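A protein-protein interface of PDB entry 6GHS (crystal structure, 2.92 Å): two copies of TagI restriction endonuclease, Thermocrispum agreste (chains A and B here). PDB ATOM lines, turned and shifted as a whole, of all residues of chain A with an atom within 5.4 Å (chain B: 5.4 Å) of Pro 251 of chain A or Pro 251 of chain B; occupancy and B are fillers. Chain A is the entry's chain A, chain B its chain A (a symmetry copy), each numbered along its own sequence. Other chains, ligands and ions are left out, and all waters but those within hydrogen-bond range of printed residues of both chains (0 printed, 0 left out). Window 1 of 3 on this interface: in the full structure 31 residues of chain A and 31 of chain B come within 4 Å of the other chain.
The side-chain hydroxyl of Tyr 224 of chain A sits at hydrogen-bond distance from the side-chain amide oxygen of Gln 226 of chain A, at 2.9 Å. O of Ile 217 of chain A is in hydrogen-bond range of N of Tyr 224 of chain A (2.8 Å). O of Ile 217 of chain B lies within hydrogen-bond range of N of Tyr 224 of chain B. OH of Tyr 224 of chain B sits at hydrogen-bond distance from OE1 of Gln 226 of chain B (2.9 Å).
N of Asn 252 of chain A is in hydrogen-bond range of OD1 of Asn 252 of chain B, at 2.8 Å. The side-chain amide oxygen (OD1) of Asn 252 of chain A lies close to the backbone nitrogen (N) of Pro 251 of chain B, 3.2 Å away. N of Pro 251 of chain A lies close to OD1 of Asn 252 of chain B, 3.2 Å away.
Tyr 224 of chain A touches Val 255 of chain B, and with the chains exchanged Val 255 of chain A touches Tyr 224 of chain B. Cys 250 of chain A touches Asn 252 of chain B, and with the chains exchanged Asn 252 of chain A touches Cys 250 of chain B. Pro 251 of chain A touches Asn 252 of chain B, and with the chains exchanged Asn 252 of chain A touches Pro 251 of chain B. Asn 252 of chain B touches its own counterpart, Asn 252 of chain A. Positions printed for both chains: 217, 224, 225, 226, 249, 250, 251, 252, 253, 254 and 255.
Ile 217 of chain A touches Asn 252 of chain B (CD1 to ND2, 3.5 Å). Val 255 of chain B touches Tyr 224 of chain A (CG1 to CD2, 3.8 Å). Cys 250 of chain A touches Asn 252 of chain B (CB to OD1, 3.8 Å). Pro 251 of chain A touches Pro 251 of chain B (CB to CB, 3.7 Å). Asn 252 of chain A touches Ile 217 of chain B (ND2 to CD1, 3.5 Å). OD1 of Asn 252 of chain A touches CB of Cys 250 of chain B, at 3.8 Å. CD2 of Tyr 224 of chain B touches CG1 of Val 255 of chain A (3.8 Å).
Of the printed residues of chain A, Ile 217 of chain B touches Asn 252 (3.5 Å). Printed residues of chain A within 4 Å of Val 255 of chain B: Tyr 224 (3.8 Å). Printed residues of chain A within 4 Å of Asn 252 of chain B: Ile 217 (3.5 Å), Cys 250 (3.8 Å), Pro 251 (3.2 Å) and Asn 252 (2.8 Å). Gln 226 of chain B touches none of the printed residues of chain A. Asp 253 of chain B touches none of the printed residues of chain A. The nearest residue of chain B that does not touch Pro 251 of chain A is Val 255 of chain B (4.1 Å). The nearest residue of chain A that does not touch Pro 251 of chain B is Val 255 of chain A (4.1 Å).
Of the 11 printed residues of chain B, 6 touch a printed residue of chain A. Hydrophobic or aromatic side chains of chain B that line the printed part of chain A: Ile 217, Tyr 224, Pro 251 and Val 255. Along chain B the printed residues that touch a printed residue of chain A span positions 217 to 255. Hydrophobic or aromatic side chains of chain A that line the printed part of chain B: Ile 217, Tyr 224, Pro 251 and Val 255. Among the printed residues, no Asp or Glu carboxylate lies within 4 Å of a Lys or Arg side-chain nitrogen of the other chain.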
ATOM      1  N   ILE A 217      -2.396  -3.423  16.659  1.00  0.00           N
ATOM      2  CA  ILE A 217      -2.209  -4.532  15.759  1.00  0.00           C
ATOM      3  C   ILE A 217      -3.612  -4.915  15.315  1.00  0.00           C
ATOM      4  O   ILE A 217      -4.467  -5.218  16.147  1.00  0.00           O
ATOM      5  CB  ILE A 217      -1.530  -5.705  16.490  1.00  0.00           C
ATOM      6  CG1 ILE A 217      -0.157  -5.293  17.030  1.00  0.00           C
ATOM      7  CG2 ILE A 217      -1.393  -6.919  15.593  1.00  0.00           C
ATOM      8  CD1 ILE A 217       0.877  -5.016  15.962  1.00  0.00           C
ATOM      9  N   TYR A 224      -5.784  -6.092  18.398  1.00  0.00           N
ATOM     10  CA  TYR A 224      -5.042  -7.036  19.219  1.00  0.00           C
ATOM     11  C   TYR A 224      -3.956  -6.356  20.061  1.00  0.00           C
ATOM     12  O   TYR A 224      -3.202  -5.528  19.563  1.00  0.00           O
ATOM     13  CB  TYR A 224      -4.378  -8.084  18.330  1.00  0.00           C
ATOM     14  CG  TYR A 224      -3.506  -9.007  19.131  1.00  0.00           C
ATOM     15  CD1 TYR A 224      -4.060 -10.059  19.842  1.00  0.00           C
ATOM     16  CD2 TYR A 224      -2.140  -8.795  19.237  1.00  0.00           C
ATOM     17  CE1 TYR A 224      -3.278 -10.901  20.608  1.00  0.00           C
ATOM     18  CE2 TYR A 224      -1.357  -9.631  20.010  1.00  0.00           C
ATOM     19  CZ  TYR A 224      -1.936 -10.683  20.687  1.00  0.00           C
ATOM     20  OH  TYR A 224      -1.178 -11.508  21.453  1.00  0.00           O
ATOM     21  N   SER A 225      -3.837  -6.744  21.324  1.00  0.00           N
ATOM     22  CA  SER A 225      -2.753  -6.246  22.165  1.00  0.00           C
ATOM     23  C   SER A 225      -2.449  -7.240  23.274  1.00  0.00           C
ATOM     24  O   SER A 225      -3.080  -8.299  23.360  1.00  0.00           O
ATOM     25  CB  SER A 225      -3.108  -4.871  22.739  1.00  0.00           C
ATOM     26  OG  SER A 225      -4.154  -4.947  23.694  1.00  0.00           O
ATOM     27  N   GLN A 226      -1.466  -6.907  24.101  1.00  0.00           N
ATOM     28  CA  GLN A 226      -1.072  -7.739  25.216  1.00  0.00           C
ATOM     29  C   GLN A 226      -1.110  -6.929  26.510  1.00  0.00           C
ATOM     30  O   GLN A 226      -0.680  -5.783  26.558  1.00  0.00           O
ATOM     31  CB  GLN A 226       0.321  -8.348  24.963  1.00  0.00           C
ATOM     32  CG  GLN A 226       0.293  -9.767  24.383  1.00  0.00           C
ATOM     33  CD  GLN A 226       1.525 -10.122  23.553  1.00  0.00           C
ATOM     34  OE1 GLN A 226       1.404 -10.683  22.464  1.00  0.00           O
ATOM     35  NE2 GLN A 226       2.713  -9.795  24.061  1.00  0.00           N
ATOM     36  N   LEU A 249       0.256  -3.166  25.710  1.00  0.00           N
ATOM     37  CA  LEU A 249       1.413  -3.067  24.808  1.00  0.00           C
ATOM     38  C   LEU A 249       1.284  -3.936  23.565  1.00  0.00           C
ATOM     39  O   LEU A 249       0.639  -4.977  23.605  1.00  0.00           O
ATOM     40  CB  LEU A 249       2.671  -3.535  25.513  1.00  0.00           C
ATOM     41  CG  LEU A 249       3.075  -2.864  26.807  1.00  0.00           C
ATOM     42  CD1 LEU A 249       4.307  -3.573  27.346  1.00  0.00           C
ATOM     43  CD2 LEU A 249       3.368  -1.396  26.580  1.00  0.00           C
ATOM     44  N   CYS A 250       1.968  -3.544  22.488  1.00  0.00           N
ATOM     45  CA  CYS A 250       2.070  -4.382  21.300  1.00  0.00           C
ATOM     46  C   CYS A 250       3.028  -5.507  21.644  1.00  0.00           C
ATOM     47  O   CYS A 250       3.815  -5.373  22.588  1.00  0.00           O
ATOM     48  CB  CYS A 250       2.589  -3.606  20.091  1.00  0.00           C
ATOM     49  SG  CYS A 250       4.200  -2.872  20.368  1.00  0.00           S
ATOM     50  N   PRO A 251       2.967  -6.625  20.907  1.00  0.00           N
ATOM     51  CA  PRO A 251       3.864  -7.753  21.200  1.00  0.00           C
ATOM     52  C   PRO A 251       5.351  -7.434  21.241  1.00  0.00           C
ATOM     53  O   PRO A 251       6.032  -7.974  22.102  1.00  0.00           O
ATOM     54  CB  PRO A 251       3.569  -8.723  20.075  1.00  0.00           C
ATOM     55  CG  PRO A 251       2.131  -8.481  19.792  1.00  0.00           C
ATOM     56  CD  PRO A 251       1.884  -7.020  19.992  1.00  0.00           C
ATOM     57  N   ASN A 252       5.830  -6.561  20.342  1.00  0.00           N
ATOM     58  CA  ASN A 252       7.255  -6.144  20.303  1.00  0.00           C
ATOM     59  C   ASN A 252       7.652  -5.416  21.580  1.00  0.00           C
ATOM     60  O   ASN A 252       8.654  -5.765  22.199  1.00  0.00           O
ATOM     61  CB  ASN A 252       7.585  -5.252  19.081  1.00  0.00           C
ATOM     62  CG  ASN A 252       7.611  -6.018  17.762  1.00  0.00           C
ATOM     63  OD1 ASN A 252       7.247  -7.182  17.698  1.00  0.00           O
ATOM     64  ND2 ASN A 252       8.027  -5.349  16.696  1.00  0.00           N
ATOM     65  N   ASP A 253       6.864  -4.429  21.984  1.00  0.00           N
ATOM     66  CA  ASP A 253       7.189  -3.689  23.201  1.00  0.00           C
ATOM     67  C   ASP A 253       7.047  -4.509  24.479  1.00  0.00           C
ATOM     68  O   ASP A 253       7.823  -4.303  25.410  1.00  0.00           O
ATOM     69  CB  ASP A 253       6.412  -2.370  23.294  1.00  0.00           C
ATOM     70  CG  ASP A 253       6.884  -1.344  22.266  1.00  0.00           C
ATOM     71  OD1 ASP A 253       8.084  -1.305  21.947  1.00  0.00           O
ATOM     72  OD2 ASP A 253       6.057  -0.571  21.757  1.00  0.00           O
ATOM     73  N   HIS A 254       6.111  -5.458  24.518  1.00  0.00           N
ATOM     74  CA  HIS A 254       6.029  -6.405  25.655  1.00  0.00           C
ATOM     75  C   HIS A 254       7.396  -7.085  25.897  1.00  0.00           C
ATOM     76  O   HIS A 254       7.904  -7.091  27.018  1.00  0.00           O
ATOM     77  CB  HIS A 254       4.929  -7.463  25.429  1.00  0.00           C
ATOM     78  CG  HIS A 254       4.541  -8.228  26.663  1.00  0.00           C
ATOM     79  ND1 HIS A 254       3.428  -9.035  26.708  1.00  0.00           N
ATOM     80  CD2 HIS A 254       5.111  -8.309  27.891  1.00  0.00           C
ATOM     81  CE1 HIS A 254       3.327  -9.581  27.907  1.00  0.00           C
ATOM     82  NE2 HIS A 254       4.338  -9.159  28.644  1.00  0.00           N
ATOM     83  N   VAL A 255       7.993  -7.610  24.834  1.00  0.00           N
ATOM     84  CA  VAL A 255       9.248  -8.341  24.926  1.00  0.00           C
ATOM     85  C   VAL A 255      10.371  -7.457  25.448  1.00  0.00           C
ATOM     86  O   VAL A 255      11.137  -7.860  26.331  1.00  0.00           O
ATOM     87  CB  VAL A 255       9.655  -8.889  23.550  1.00  0.00           C
ATOM     88  CG1 VAL A 255      11.072  -9.450  23.565  1.00  0.00           C
ATOM     89  CG2 VAL A 255       8.681  -9.972  23.112  1.00  0.00           C
ATOM     90  N   ILE B 217      14.602  -6.878  17.075  1.00  0.00           N
ATOM     91  CA  ILE B 217      14.255  -6.501  18.421  1.00  0.00           C
ATOM     92  C   ILE B 217      15.530  -6.706  19.225  1.00  0.00           C
ATOM     93  O   ILE B 217      16.079  -7.808  19.250  1.00  0.00           O
ATOM     94  CB  ILE B 217      13.125  -7.400  18.954  1.00  0.00           C
ATOM     95  CG1 ILE B 217      11.869  -7.273  18.086  1.00  0.00           C
ATOM     96  CG2 ILE B 217      12.792  -7.083  20.398  1.00  0.00           C
ATOM     97  CD1 ILE B 217      11.190  -5.924  18.162  1.00  0.00           C
ATOM     98  N   TYR B 224      16.617 -10.504  19.175  1.00  0.00           N
ATOM     99  CA  TYR B 224      15.480 -11.368  19.457  1.00  0.00           C
ATOM    100  C   TYR B 224      14.518 -11.480  18.269  1.00  0.00           C
ATOM    101  O   TYR B 224      14.163 -10.482  17.652  1.00  0.00           O
ATOM    102  CB  TYR B 224      14.706 -10.829  20.656  1.00  0.00           C
ATOM    103  CG  TYR B 224      13.458 -11.627  20.905  1.00  0.00           C
ATOM    104  CD1 TYR B 224      13.519 -12.838  21.574  1.00  0.00           C
ATOM    105  CD2 TYR B 224      12.228 -11.211  20.416  1.00  0.00           C
ATOM    106  CE1 TYR B 224      12.386 -13.600  21.786  1.00  0.00           C
ATOM    107  CE2 TYR B 224      11.097 -11.976  20.620  1.00  0.00           C
ATOM    108  CZ  TYR B 224      11.187 -13.166  21.310  1.00  0.00           C
ATOM    109  OH  TYR B 224      10.082 -13.928  21.512  1.00  0.00           O
ATOM    110  N   SER B 225      14.051 -12.687  17.978  1.00  0.00           N
ATOM    111  CA  SER B 225      13.036 -12.873  16.947  1.00  0.00           C
ATOM    112  C   SER B 225      12.238 -14.139  17.217  1.00  0.00           C
ATOM    113  O   SER B 225      12.485 -14.839  18.204  1.00  0.00           O
ATOM    114  CB  SER B 225      13.682 -12.913  15.559  1.00  0.00           C
ATOM    115  OG  SER B 225      14.455 -14.087  15.366  1.00  0.00           O
ATOM    116  N   GLN B 226      11.268 -14.411  16.352  1.00  0.00           N
ATOM    117  CA  GLN B 226      10.436 -15.589  16.463  1.00  0.00           C
ATOM    118  C   GLN B 226      10.478 -16.381  15.158  1.00  0.00           C
ATOM    119  O   GLN B 226      10.420 -15.821  14.069  1.00  0.00           O
ATOM    120  CB  GLN B 226       8.997 -15.192  16.845  1.00  0.00           C
ATOM    121  CG  GLN B 226       8.696 -15.282  18.346  1.00  0.00           C
ATOM    122  CD  GLN B 226       7.593 -14.335  18.815  1.00  0.00           C
ATOM    123  OE1 GLN B 226       7.738 -13.666  19.838  1.00  0.00           O
ATOM    124  NE2 GLN B 226       6.490 -14.273  18.069  1.00  0.00           N
ATOM    125  N   LEU B 249      10.510 -13.735  12.049  1.00  0.00           N
ATOM    126  CA  LEU B 249       9.631 -12.564  12.177  1.00  0.00           C
ATOM    127  C   LEU B 249       9.716 -11.890  13.539  1.00  0.00           C
ATOM    128  O   LEU B 249       9.991 -12.549  14.535  1.00  0.00           O
ATOM    129  CB  LEU B 249       8.180 -12.974  12.007  1.00  0.00           C
ATOM    130  CG  LEU B 249       7.767 -13.688  10.739  1.00  0.00           C
ATOM    131  CD1 LEU B 249       6.299 -14.062  10.861  1.00  0.00           C
ATOM    132  CD2 LEU B 249       7.988 -12.802   9.531  1.00  0.00           C
ATOM    133  N   CYS B 250       9.401 -10.595  13.587  1.00  0.00           N
ATOM    134  CA  CYS B 250       9.271  -9.885  14.853  1.00  0.00           C
ATOM    135  C   CYS B 250       7.967 -10.346  15.476  1.00  0.00           C
ATOM    136  O   CYS B 250       7.097 -10.860  14.764  1.00  0.00           O
ATOM    137  CB  CYS B 250       9.251  -8.370  14.664  1.00  0.00           C
ATOM    138  SG  CYS B 250       7.923  -7.812  13.599  1.00  0.00           S
ATOM    139  N   PRO B 251       7.818 -10.189  16.799  1.00  0.00           N
ATOM    140  CA  PRO B 251       6.580 -10.626  17.460  1.00  0.00           C
ATOM    141  C   PRO B 251       5.283 -10.074  16.888  1.00  0.00           C
ATOM    142  O   PRO B 251       4.320 -10.825  16.815  1.00  0.00           O
ATOM    143  CB  PRO B 251       6.768 -10.147  18.885  1.00  0.00           C
ATOM    144  CG  PRO B 251       8.237 -10.247  19.082  1.00  0.00           C
ATOM    145  CD  PRO B 251       8.879  -9.897  17.777  1.00  0.00           C
ATOM    146  N   ASN B 252       5.272  -8.797  16.476  1.00  0.00           N
ATOM    147  CA  ASN B 252       4.079  -8.155  15.870  1.00  0.00           C
ATOM    148  C   ASN B 252       3.693  -8.832  14.561  1.00  0.00           C
ATOM    149  O   ASN B 252       2.535  -9.199  14.378  1.00  0.00           O
ATOM    150  CB  ASN B 252       4.274  -6.639  15.623  1.00  0.00           C
ATOM    151  CG  ASN B 252       4.262  -5.811  16.904  1.00  0.00           C
ATOM    152  OD1 ASN B 252       4.256  -6.344  18.002  1.00  0.00           O
ATOM    153  ND2 ASN B 252       4.279  -4.494  16.758  1.00  0.00           N
ATOM    154  N   ASP B 253       4.656  -9.018  13.668  1.00  0.00           N
ATOM    155  CA  ASP B 253       4.351  -9.662  12.393  1.00  0.00           C
ATOM    156  C   ASP B 253       3.992 -11.139  12.516  1.00  0.00           C
ATOM    157  O   ASP B 253       3.157 -11.616  11.751  1.00  0.00           O
ATOM    158  CB  ASP B 253       5.464  -9.441  11.361  1.00  0.00           C
ATOM    159  CG  ASP B 253       5.532  -7.993  10.880  1.00  0.00           C
ATOM    160  OD1 ASP B 253       4.485  -7.335  10.774  1.00  0.00           O
ATOM    161  OD2 ASP B 253       6.637  -7.494  10.613  1.00  0.00           O
ATOM    162  N   HIS B 254       4.566 -11.848  13.488  1.00  0.00           N
ATOM    163  CA  HIS B 254       4.139 -13.237  13.777  1.00  0.00           C
ATOM    164  C   HIS B 254       2.609 -13.303  13.989  1.00  0.00           C
ATOM    165  O   HIS B 254       1.924 -14.113  13.365  1.00  0.00           O
ATOM    166  CB  HIS B 254       4.883 -13.814  14.999  1.00  0.00           C
ATOM    167  CG  HIS B 254       4.778 -15.306  15.142  1.00  0.00           C
ATOM    168  ND1 HIS B 254       5.560 -16.017  16.022  1.00  0.00           N
ATOM    169  CD2 HIS B 254       3.992 -16.220  14.520  1.00  0.00           C
ATOM    170  CE1 HIS B 254       5.261 -17.302  15.939  1.00  0.00           C
ATOM    171  NE2 HIS B 254       4.310 -17.451  15.037  1.00  0.00           N
ATOM    172  N   VAL B 255       2.090 -12.421  14.834  1.00  0.00           N
ATOM    173  CA  VAL B 255       0.678 -12.413  15.183  1.00  0.00           C
ATOM    174  C   VAL B 255      -0.197 -12.155  13.965  1.00  0.00           C
ATOM    175  O   VAL B 255      -1.200 -12.844  13.747  1.00  0.00           O
ATOM    176  CB  VAL B 255       0.388 -11.330  16.233  1.00  0.00           C
ATOM    177  CG1 VAL B 255      -1.110 -11.137  16.442  1.00  0.00           C
ATOM    178  CG2 VAL B 255       1.045 -11.696  17.554  1.00  0.00           C
